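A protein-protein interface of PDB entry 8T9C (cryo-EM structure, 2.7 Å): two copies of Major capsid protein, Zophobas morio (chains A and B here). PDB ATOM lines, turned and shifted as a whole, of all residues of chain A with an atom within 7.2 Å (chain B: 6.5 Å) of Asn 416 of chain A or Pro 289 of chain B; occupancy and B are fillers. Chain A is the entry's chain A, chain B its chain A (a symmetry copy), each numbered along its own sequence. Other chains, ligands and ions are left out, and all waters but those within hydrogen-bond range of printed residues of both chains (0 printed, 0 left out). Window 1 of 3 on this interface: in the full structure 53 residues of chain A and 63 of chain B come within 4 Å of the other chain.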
ATOM      1  N   PRO A 413      12.541   8.322 -35.568  1.00  0.00           N
ATOM      2  CA  PRO A 413      13.133   7.891 -34.301  1.00  0.00           C
ATOM      3  C   PRO A 413      14.555   7.394 -34.498  1.00  0.00           C
ATOM      4  O   PRO A 413      15.008   7.134 -35.614  1.00  0.00           O
ATOM      5  CB  PRO A 413      12.210   6.756 -33.853  1.00  0.00           C
ATOM      6  CG  PRO A 413      11.676   6.206 -35.124  1.00  0.00           C
ATOM      7  CD  PRO A 413      11.512   7.383 -36.043  1.00  0.00           C
ATOM      8  N   VAL A 414      15.268   7.277 -33.384  1.00  0.00           N
ATOM      9  CA  VAL A 414      16.566   6.612 -33.390  1.00  0.00           C
ATOM     10  C   VAL A 414      16.300   5.131 -33.628  1.00  0.00           C
ATOM     11  O   VAL A 414      15.572   4.505 -32.846  1.00  0.00           O
ATOM     12  CB  VAL A 414      17.332   6.852 -32.079  1.00  0.00           C
ATOM     13  CG1 VAL A 414      18.638   6.078 -32.078  1.00  0.00           C
ATOM     14  CG2 VAL A 414      17.589   8.334 -31.883  1.00  0.00           C
ATOM     15  N   PRO A 415      16.852   4.536 -34.685  1.00  0.00           N
ATOM     16  CA  PRO A 415      16.514   3.142 -35.019  1.00  0.00           C
ATOM     17  C   PRO A 415      17.009   2.183 -33.947  1.00  0.00           C
ATOM     18  O   PRO A 415      18.211   2.087 -33.687  1.00  0.00           O
ATOM     19  CB  PRO A 415      17.228   2.916 -36.358  1.00  0.00           C
ATOM     20  CG  PRO A 415      17.498   4.289 -36.888  1.00  0.00           C
ATOM     21  CD  PRO A 415      17.756   5.129 -35.680  1.00  0.00           C
ATOM     22  N   ASN A 416      16.069   1.467 -33.327  1.00  0.00           N
ATOM     23  CA  ASN A 416      16.411   0.530 -32.263  1.00  0.00           C
ATOM     24  C   ASN A 416      17.210  -0.659 -32.774  1.00  0.00           C
ATOM     25  O   ASN A 416      17.837  -1.357 -31.972  1.00  0.00           O
ATOM     26  CB  ASN A 416      15.142   0.036 -31.567  1.00  0.00           C
ATOM     27  CG  ASN A 416      14.743   0.912 -30.405  1.00  0.00           C
ATOM     28  OD1 ASN A 416      15.364   1.941 -30.148  1.00  0.00           O
ATOM     29  ND2 ASN A 416      13.697   0.510 -29.695  1.00  0.00           N
ATOM     30  N   ASN A 417      17.194  -0.915 -34.085  1.00  0.00           N
ATOM     31  CA  ASN A 417      17.978  -2.014 -34.632  1.00  0.00           C
ATOM     32  C   ASN A 417      19.474  -1.760 -34.526  1.00  0.00           C
ATOM     33  O   ASN A 417      20.260  -2.710 -34.593  1.00  0.00           O
ATOM     34  CB  ASN A 417      17.584  -2.269 -36.087  1.00  0.00           C
ATOM     35  CG  ASN A 417      18.245  -1.308 -37.048  1.00  0.00           C
ATOM     36  OD1 ASN A 417      18.130  -0.094 -36.908  1.00  0.00           O
ATOM     37  ND2 ASN A 417      18.945  -1.851 -38.034  1.00  0.00           N
ATOM     38  N   LEU A 418      19.884  -0.503 -34.358  1.00  0.00           N
ATOM     39  CA  LEU A 418      21.288  -0.184 -34.149  1.00  0.00           C
ATOM     40  C   LEU A 418      21.712  -0.339 -32.698  1.00  0.00           C
ATOM     41  O   LEU A 418      22.901  -0.200 -32.395  1.00  0.00           O
ATOM     42  CB  LEU A 418      21.572   1.242 -34.612  1.00  0.00           C
ATOM     43  CG  LEU A 418      21.188   1.556 -36.054  1.00  0.00           C
ATOM     44  CD1 LEU A 418      21.425   3.014 -36.344  1.00  0.00           C
ATOM     45  CD2 LEU A 418      22.000   0.692 -37.000  1.00  0.00           C
ATOM     46  N   ILE A 419      20.772  -0.625 -31.802  1.00  0.00           N
ATOM     47  CA  ILE A 419      21.048  -0.706 -30.373  1.00  0.00           C
ATOM     48  C   ILE A 419      20.661  -2.080 -29.842  1.00  0.00           C
ATOM     49  O   ILE A 419      21.276  -2.591 -28.902  1.00  0.00           O
ATOM     50  CB  ILE A 419      20.297   0.403 -29.616  1.00  0.00           C
ATOM     51  CG1 ILE A 419      20.521   1.754 -30.293  1.00  0.00           C
ATOM     52  CG2 ILE A 419      20.726   0.453 -28.170  1.00  0.00           C
ATOM     53  CD1 ILE A 419      19.589   2.840 -29.812  1.00  0.00           C
ATOM     54  N   THR A 420      19.654  -2.695 -30.453  1.00  0.00           N
ATOM     55  CA  THR A 420      19.033  -3.887 -29.904  1.00  0.00           C
ATOM     56  C   THR A 420      19.016  -4.992 -30.953  1.00  0.00           C
ATOM     57  O   THR A 420      18.904  -4.728 -32.152  1.00  0.00           O
ATOM     58  CB  THR A 420      17.595  -3.589 -29.444  1.00  0.00           C
ATOM     59  OG1 THR A 420      17.589  -2.440 -28.591  1.00  0.00           O
ATOM     60  CG2 THR A 420      17.061  -4.723 -28.645  1.00  0.00           C
ATOM     61  N   GLN A 421      19.129  -6.236 -30.488  1.00  0.00           N
ATOM     62  CA  GLN A 421      18.924  -7.405 -31.335  1.00  0.00           C
ATOM     63  C   GLN A 421      17.477  -7.873 -31.348  1.00  0.00           C
ATOM     64  O   GLN A 421      17.171  -8.882 -31.987  1.00  0.00           O
ATOM     65  CB  GLN A 421      19.809  -8.562 -30.871  1.00  0.00           C
ATOM     66  CG  GLN A 421      19.425  -9.102 -29.503  1.00  0.00           C
ATOM     67  CD  GLN A 421      20.019 -10.468 -29.215  1.00  0.00           C
ATOM     68  OE1 GLN A 421      19.405 -11.495 -29.503  1.00  0.00           O
ATOM     69  NE2 GLN A 421      21.219 -10.487 -28.644  1.00  0.00           N
ATOM     70  N   ASN A 422      16.596  -7.175 -30.643  1.00  0.00           N
ATOM     71  CA  ASN A 422      15.204  -7.554 -30.473  1.00  0.00           C
ATOM     72  C   ASN A 422      14.267  -6.765 -31.379  1.00  0.00           C
ATOM     73  O   ASN A 422      13.047  -6.865 -31.227  1.00  0.00           O
ATOM     74  CB  ASN A 422      14.814  -7.353 -29.006  1.00  0.00           C
ATOM     75  CG  ASN A 422      13.606  -8.137 -28.615  1.00  0.00           C
ATOM     76  OD1 ASN A 422      13.338  -9.201 -29.168  1.00  0.00           O
ATOM     77  ND2 ASN A 422      12.860  -7.624 -27.644  1.00  0.00           N
ATOM     78  N   TYR A 423      14.813  -5.982 -32.312  1.00  0.00           N
ATOM     79  CA  TYR A 423      14.005  -5.049 -33.090  1.00  0.00           C
ATOM     80  C   TYR A 423      12.942  -5.757 -33.920  1.00  0.00           C
ATOM     81  O   TYR A 423      11.862  -5.203 -34.147  1.00  0.00           O
ATOM     82  CB  TYR A 423      14.906  -4.207 -33.993  1.00  0.00           C
ATOM     83  CG  TYR A 423      15.755  -5.008 -34.953  1.00  0.00           C
ATOM     84  CD1 TYR A 423      16.960  -5.563 -34.547  1.00  0.00           C
ATOM     85  CD2 TYR A 423      15.350  -5.211 -36.264  1.00  0.00           C
ATOM     86  CE1 TYR A 423      17.738  -6.293 -35.418  1.00  0.00           C
ATOM     87  CE2 TYR A 423      16.123  -5.942 -37.144  1.00  0.00           C
ATOM     88  CZ  TYR A 423      17.314  -6.480 -36.715  1.00  0.00           C
ATOM     89  OH  TYR A 423      18.085  -7.208 -37.588  1.00  0.00           O
ATOM     90  N   TYR A 548      16.690  12.300 -27.445  1.00  0.00           N
ATOM     91  CA  TYR A 548      18.116  12.107 -27.246  1.00  0.00           C
ATOM     92  C   TYR A 548      18.810  13.449 -27.061  1.00  0.00           C
ATOM     93  O   TYR A 548      18.305  14.499 -27.464  1.00  0.00           O
ATOM     94  CB  TYR A 548      18.740  11.350 -28.422  1.00  0.00           C
ATOM     95  CG  TYR A 548      18.592   9.850 -28.334  1.00  0.00           C
ATOM     96  CD1 TYR A 548      17.346   9.248 -28.445  1.00  0.00           C
ATOM     97  CD2 TYR A 548      19.696   9.033 -28.140  1.00  0.00           C
ATOM     98  CE1 TYR A 548      17.204   7.878 -28.362  1.00  0.00           C
ATOM     99  CE2 TYR A 548      19.564   7.662 -28.058  1.00  0.00           C
ATOM    100  CZ  TYR A 548      18.317   7.091 -28.171  1.00  0.00           C
ATOM    101  OH  TYR A 548      18.178   5.725 -28.090  1.00  0.00           O
ATOM    102  N   ALA A 556       9.681   9.287 -30.638  1.00  0.00           N
ATOM    103  CA  ALA A 556       9.556   7.904 -30.208  1.00  0.00           C
ATOM    104  C   ALA A 556       9.209   7.029 -31.405  1.00  0.00           C
ATOM    105  O   ALA A 556       8.548   7.473 -32.347  1.00  0.00           O
ATOM    106  CB  ALA A 556       8.488   7.779 -29.122  1.00  0.00           C
ATOM    107  N   ASN A 557       9.672   5.778 -31.378  1.00  0.00           N
ATOM    108  CA  ASN A 557       9.384   4.878 -32.487  1.00  0.00           C
ATOM    109  C   ASN A 557       7.902   4.532 -32.573  1.00  0.00           C
ATOM    110  O   ASN A 557       7.440   4.089 -33.630  1.00  0.00           O
ATOM    111  CB  ASN A 557      10.234   3.611 -32.374  1.00  0.00           C
ATOM    112  CG  ASN A 557       9.956   2.824 -31.111  1.00  0.00           C
ATOM    113  OD1 ASN A 557       9.206   3.261 -30.240  1.00  0.00           O
ATOM    114  ND2 ASN A 557      10.572   1.653 -31.004  1.00  0.00           N
ATOM    115  N   THR A 558       7.145   4.733 -31.493  1.00  0.00           N
ATOM    116  CA  THR A 558       5.698   4.571 -31.559  1.00  0.00           C
ATOM    117  C   THR A 558       5.037   5.668 -32.382  1.00  0.00           C
ATOM    118  O   THR A 558       3.856   5.542 -32.725  1.00  0.00           O
ATOM    119  CB  THR A 558       5.102   4.550 -30.151  1.00  0.00           C
ATOM    120  OG1 THR A 558       5.516   5.719 -29.435  1.00  0.00           O
ATOM    121  CG2 THR A 558       5.557   3.313 -29.402  1.00  0.00           C
ATOM    122  N   LYS A 559       5.764   6.736 -32.698  1.00  0.00           N
ATOM    123  CA  LYS A 559       5.271   7.785 -33.577  1.00  0.00           C
ATOM    124  C   LYS A 559       5.648   7.555 -35.033  1.00  0.00           C
ATOM    125  O   LYS A 559       5.374   8.420 -35.870  1.00  0.00           O
ATOM    126  CB  LYS A 559       5.797   9.147 -33.120  1.00  0.00           C
ATOM    127  CG  LYS A 559       5.302   9.574 -31.755  1.00  0.00           C
ATOM    128  CD  LYS A 559       3.810   9.826 -31.767  1.00  0.00           C
ATOM    129  CE  LYS A 559       3.340  10.413 -30.452  1.00  0.00           C
ATOM    130  NZ  LYS A 559       1.869  10.636 -30.447  1.00  0.00           N
ATOM    131  N   PRO B 208      23.917  -5.634 -32.408  1.00  0.00           N
ATOM    132  CA  PRO B 208      24.881  -4.655 -32.918  1.00  0.00           C
ATOM    133  C   PRO B 208      25.839  -4.201 -31.827  1.00  0.00           C
ATOM    134  O   PRO B 208      25.663  -4.480 -30.640  1.00  0.00           O
ATOM    135  CB  PRO B 208      23.990  -3.506 -33.388  1.00  0.00           C
ATOM    136  CG  PRO B 208      22.817  -3.575 -32.472  1.00  0.00           C
ATOM    137  CD  PRO B 208      22.587  -5.038 -32.195  1.00  0.00           C
ATOM    138  N   ILE B 285      10.576   2.292 -16.369  1.00  0.00           N
ATOM    139  CA  ILE B 285      11.583   2.619 -17.376  1.00  0.00           C
ATOM    140  C   ILE B 285      11.594   1.577 -18.484  1.00  0.00           C
ATOM    141  O   ILE B 285      11.873   1.894 -19.647  1.00  0.00           O
ATOM    142  CB  ILE B 285      12.970   2.758 -16.714  1.00  0.00           C
ATOM    143  CG1 ILE B 285      12.960   3.896 -15.695  1.00  0.00           C
ATOM    144  CG2 ILE B 285      14.050   3.006 -17.752  1.00  0.00           C
ATOM    145  CD1 ILE B 285      12.679   5.249 -16.293  1.00  0.00           C
ATOM    146  N   ARG B 286      11.279   0.325 -18.150  1.00  0.00           N
ATOM    147  CA  ARG B 286      11.341  -0.755 -19.128  1.00  0.00           C
ATOM    148  C   ARG B 286      10.360  -0.541 -20.277  1.00  0.00           C
ATOM    149  O   ARG B 286      10.612  -0.994 -21.399  1.00  0.00           O
ATOM    150  CB  ARG B 286      11.071  -2.090 -18.434  1.00  0.00           C
ATOM    151  CG  ARG B 286      11.215  -3.313 -19.316  1.00  0.00           C
ATOM    152  CD  ARG B 286      11.098  -4.593 -18.509  1.00  0.00           C
ATOM    153  NE  ARG B 286       9.830  -4.668 -17.794  1.00  0.00           N
ATOM    154  CZ  ARG B 286       9.693  -5.100 -16.549  1.00  0.00           C
ATOM    155  NH1 ARG B 286      10.731  -5.519 -15.845  1.00  0.00           N
ATOM    156  NH2 ARG B 286       8.485  -5.111 -15.997  1.00  0.00           N
ATOM    157  N   SER B 287       9.248   0.149 -20.027  1.00  0.00           N
ATOM    158  CA  SER B 287       8.212   0.315 -21.037  1.00  0.00           C
ATOM    159  C   SER B 287       8.389   1.562 -21.892  1.00  0.00           C
ATOM    160  O   SER B 287       7.617   1.755 -22.837  1.00  0.00           O
ATOM    161  CB  SER B 287       6.835   0.356 -20.373  1.00  0.00           C
ATOM    162  OG  SER B 287       6.635  -0.770 -19.541  1.00  0.00           O
ATOM    163  N   ILE B 288       9.371   2.409 -21.596  1.00  0.00           N
ATOM    164  CA  ILE B 288       9.540   3.659 -22.333  1.00  0.00           C
ATOM    165  C   ILE B 288      10.032   3.335 -23.740  1.00  0.00           C
ATOM    166  O   ILE B 288      11.077   2.689 -23.898  1.00  0.00           O
ATOM    167  CB  ILE B 288      10.489   4.615 -21.598  1.00  0.00           C
ATOM    168  CG1 ILE B 288       9.896   5.003 -20.244  1.00  0.00           C
ATOM    169  CG2 ILE B 288      10.731   5.860 -22.422  1.00  0.00           C
ATOM    170  CD1 ILE B 288      10.818   5.838 -19.388  1.00  0.00           C
ATOM    171  N   PRO B 289       9.307   3.758 -24.781  1.00  0.00           N
ATOM    172  CA  PRO B 289       9.625   3.291 -26.140  1.00  0.00           C
ATOM    173  C   PRO B 289      11.008   3.679 -26.624  1.00  0.00           C
ATOM    174  O   PRO B 289      11.595   2.956 -27.436  1.00  0.00           O
ATOM    175  CB  PRO B 289       8.533   3.950 -26.995  1.00  0.00           C
ATOM    176  CG  PRO B 289       7.440   4.277 -26.042  1.00  0.00           C
ATOM    177  CD  PRO B 289       8.120   4.625 -24.761  1.00  0.00           C
ATOM    178  N   PHE B 290      11.546   4.801 -26.155  1.00  0.00           N
ATOM    179  CA  PHE B 290      12.771   5.351 -26.712  1.00  0.00           C
ATOM    180  C   PHE B 290      13.981   5.184 -25.806  1.00  0.00           C
ATOM    181  O   PHE B 290      15.101   5.480 -26.237  1.00  0.00           O
ATOM    182  CB  PHE B 290      12.571   6.832 -27.035  1.00  0.00           C
ATOM    183  CG  PHE B 290      11.870   7.600 -25.953  1.00  0.00           C
ATOM    184  CD1 PHE B 290      12.585   8.166 -24.914  1.00  0.00           C
ATOM    185  CD2 PHE B 290      10.496   7.757 -25.977  1.00  0.00           C
ATOM    186  CE1 PHE B 290      11.944   8.871 -23.921  1.00  0.00           C
ATOM    187  CE2 PHE B 290       9.851   8.463 -24.987  1.00  0.00           C
ATOM    188  CZ  PHE B 290      10.576   9.019 -23.954  1.00  0.00           C
ATOM    189  N   ILE B 291      13.796   4.724 -24.573  1.00  0.00           N
ATOM    190  CA  ILE B 291      14.930   4.397 -23.719  1.00  0.00           C
ATOM    191  C   ILE B 291      15.168   2.897 -23.807  1.00  0.00           C
ATOM    192  O   ILE B 291      14.507   2.110 -23.122  1.00  0.00           O
ATOM    193  CB  ILE B 291      14.697   4.843 -22.265  1.00  0.00           C
ATOM    194  CG1 ILE B 291      14.386   6.339 -22.211  1.00  0.00           C
ATOM    195  CG2 ILE B 291      15.916   4.528 -21.414  1.00  0.00           C
ATOM    196  CD1 ILE B 291      14.355   6.905 -20.815  1.00  0.00           C
ATOM    197  N   CYS B 292      16.103   2.492 -24.661  1.00  0.00           N
ATOM    198  CA  CYS B 292      16.411   1.077 -24.808  1.00  0.00           C
ATOM    199  C   CYS B 292      17.287   0.628 -23.650  1.00  0.00           C
ATOM    200  O   CYS B 292      18.457   1.010 -23.558  1.00  0.00           O
ATOM    201  CB  CYS B 292      17.108   0.819 -26.142  1.00  0.00           C
ATOM    202  SG  CYS B 292      17.893  -0.798 -26.247  1.00  0.00           S
ATOM    203  N   SER B 443      11.819  -2.589 -36.133  1.00  0.00           N
ATOM    204  CA  SER B 443      12.368  -1.261 -35.886  1.00  0.00           C
ATOM    205  C   SER B 443      13.456  -0.897 -36.886  1.00  0.00           C
ATOM    206  O   SER B 443      13.826   0.277 -36.983  1.00  0.00           O
ATOM    207  CB  SER B 443      12.912  -1.167 -34.464  1.00  0.00           C
ATOM    208  OG  SER B 443      13.355   0.148 -34.190  1.00  0.00           O
ATOM    209  N   SER B 444      13.981  -1.876 -37.626  1.00  0.00           N
ATOM    210  CA  SER B 444      14.881  -1.576 -38.731  1.00  0.00           C
ATOM    211  C   SER B 444      14.134  -1.018 -39.932  1.00  0.00           C
ATOM    212  O   SER B 444      14.772  -0.523 -40.868  1.00  0.00           O
ATOM    213  CB  SER B 444      15.651  -2.830 -39.142  1.00  0.00           C
ATOM    214  OG  SER B 444      14.874  -3.643 -40.001  1.00  0.00           O
ATOM    215  N   ASN B 580      12.307  -3.248 -24.502  1.00  0.00           N
ATOM    216  CA  ASN B 580      11.004  -3.139 -25.138  1.00  0.00           C
ATOM    217  C   ASN B 580      11.144  -2.794 -26.618  1.00  0.00           C
ATOM    218  O   ASN B 580      12.117  -2.175 -27.055  1.00  0.00           O
ATOM    219  CB  ASN B 580      10.147  -2.085 -24.428  1.00  0.00           C
ATOM    220  CG  ASN B 580      10.529  -0.665 -24.797  1.00  0.00           C
ATOM    221  OD1 ASN B 580      10.177  -0.169 -25.866  1.00  0.00           O
ATOM    222  ND2 ASN B 580      11.242   0.001 -23.902  1.00  0.00           N
ATOM    223  N   VAL B 581      10.148  -3.212 -27.390  1.00  0.00           N
ATOM    224  CA  VAL B 581      10.022  -2.850 -28.795  1.00  0.00           C
ATOM    225  C   VAL B 581       8.729  -2.063 -28.951  1.00  0.00           C
ATOM    226  O   VAL B 581       7.636  -2.602 -28.740  1.00  0.00           O
ATOM    227  CB  VAL B 581      10.058  -4.084 -29.710  1.00  0.00           C
ATOM    228  CG1 VAL B 581      11.460  -4.650 -29.752  1.00  0.00           C
ATOM    229  CG2 VAL B 581       9.105  -5.162 -29.210  1.00  0.00           C
ATOM    230  N   TYR B 582       8.857  -0.779 -29.292  1.00  0.00           N
ATOM    231  CA  TYR B 582       7.715   0.133 -29.367  1.00  0.00           C
ATOM    232  C   TYR B 582       6.916   0.137 -28.068  1.00  0.00           C
ATOM    233  O   TYR B 582       5.687   0.227 -28.074  1.00  0.00           O
ATOM    234  CB  TYR B 582       6.812  -0.204 -30.555  1.00  0.00           C
ATOM    235  CG  TYR B 582       7.513  -0.134 -31.890  1.00  0.00           C
ATOM    236  CD1 TYR B 582       8.209  -1.222 -32.391  1.00  0.00           C
ATOM    237  CD2 TYR B 582       7.483   1.026 -32.646  1.00  0.00           C
ATOM    238  CE1 TYR B 582       8.852  -1.157 -33.608  1.00  0.00           C
ATOM    239  CE2 TYR B 582       8.119   1.099 -33.865  1.00  0.00           C
ATOM    240  CZ  TYR B 582       8.802   0.007 -34.342  1.00  0.00           C
ATOM    241  OH  TYR B 582       9.436   0.083 -35.556  1.00  0.00           O
ATOM    242  N   GLY B 583       7.615   0.045 -26.938  1.00  0.00           N
ATOM    243  CA  GLY B 583       6.970  -0.007 -25.647  1.00  0.00           C
ATOM    244  C   GLY B 583       6.314  -1.324 -25.306  1.00  0.00           C
ATOM    245  O   GLY B 583       5.514  -1.369 -24.366  1.00  0.00           O
ATOM    246  N   ARG B 584       6.624  -2.395 -26.032  1.00  0.00           N
ATOM    247  CA  ARG B 584       5.988  -3.692 -25.840  1.00  0.00           C
ATOM    248  C   ARG B 584       7.017  -4.712 -25.378  1.00  0.00           C
ATOM    249  O   ARG B 584       8.148  -4.726 -25.872  1.00  0.00           O
ATOM    250  CB  ARG B 584       5.331  -4.172 -27.135  1.00  0.00           C
ATOM    251  CG  ARG B 584       4.516  -3.117 -27.848  1.00  0.00           C
ATOM    252  CD  ARG B 584       3.185  -2.887 -27.165  1.00  0.00           C
ATOM    253  NE  ARG B 584       2.281  -4.012 -27.369  1.00  0.00           N
ATOM    254  CZ  ARG B 584       1.402  -4.090 -28.357  1.00  0.00           C
ATOM    255  NH1 ARG B 584       1.270  -3.117 -29.242  1.00  0.00           N
ATOM    256  NH2 ARG B 584       0.642  -5.175 -28.465  1.00  0.00           N
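Among the printed residues, pairs that only touch across the chains: Asn 422 of chain A with Val 581 of chain B (3.1 Å), Thr 558 of chain A with Tyr 582 of chain B (3.4 Å), Leu 418 of chain A with Pro 208 of chain B (3.4 Å), Asn 557 of chain A with Pro 289 of chain B (3.4 Å), Asn 417 of chain A with Pro 208 of chain B (3.4 Å), Tyr 548 of chain A with Phe 290 of chain B (3.6 Å), Asn 417 of chain A with Ser 444 of chain B (3.6 Å), Ile 419 of chain A with Cys 292 of chain B (3.6 Å), Ile 419 of chain A with Pro 208 of chain B (3.7 Å), Thr 420 of chain A with Pro 208 of chain B (3.7 Å), Tyr 423 of chain A with Ser 444 of chain B (3.7 Å), Ala 556 of chain A with Phe 290 of chain B (3.7 Å), Thr 558 of chain A with Pro 289 of chain B (3.9 Å), Asn 416 of chain A with Pro 289 of chain B (3.9 Å) and Asn 417 of chain A with Ser 443 of chain B (3.98 Å).
No position is printed for both chains.
Of the 19 pairs that touch across the chains among the printed residues, none has its exchanged pair printed and touching as well.
N of Asn 416 of chain A lies within hydrogen-bond range of OG of Ser 443 of chain B, at 3.1 Å.
The side-chain hydroxyl (OG1) of Thr 420 of chain A is in hydrogen-bond range of the side-chain sulfur (SG) of Cys 292 of chain B, at 2.9 Å.
O of Tyr 423 of chain A is in hydrogen-bond range of N of Ser 443 of chain B (3.3 Å).
The side-chain amide nitrogen (ND2) of Asn 557 of chain A sits close to the backbone NH (N) of Tyr 582 of chain B (3.4 Å).
Of the 16 printed residues of chain A, 11 touch a printed residue of chain B.
Of the 16 printed residues of chain B, 8 touch a printed residue of chain A.
Hydrophobic or aromatic side chains of chain B within 4 Å of the printed part of chain A: Pro 208, Pro 289, Phe 290, Val 581 and Tyr 582.
Among the printed residues, no Asp or Glu carboxylate lies within 4 Å of a Lys or Arg side-chain nitrogen of the other chain.
Asn 416 of chain A touches two residues of chain B.
Of the printed residues of chain B, Thr 558 of chain A touches Pro 289 and Tyr 582.
Ile 285 of chain B touches none of the printed residues of chain A.
Printed residues of chain A within 4 Å of Val 581 of chain B: Asn 422 (3.1 Å).
Of the printed residues of chain A, Tyr 582 of chain B touches Asn 557 (3.1 Å) and Thr 558 (3.4 Å).
The nearest residue of chain B that does not touch Asn 416 of chain A is Asn 580 of chain B (4.1 Å).
The nearest residue of chain A that does not touch Pro 289 of chain B is Ala 556 of chain A (4.4 Å).
The nearest printed residue of chain B that does not touch Leu 418 of chain A is Ser 443 of chain B (6.6 Å).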
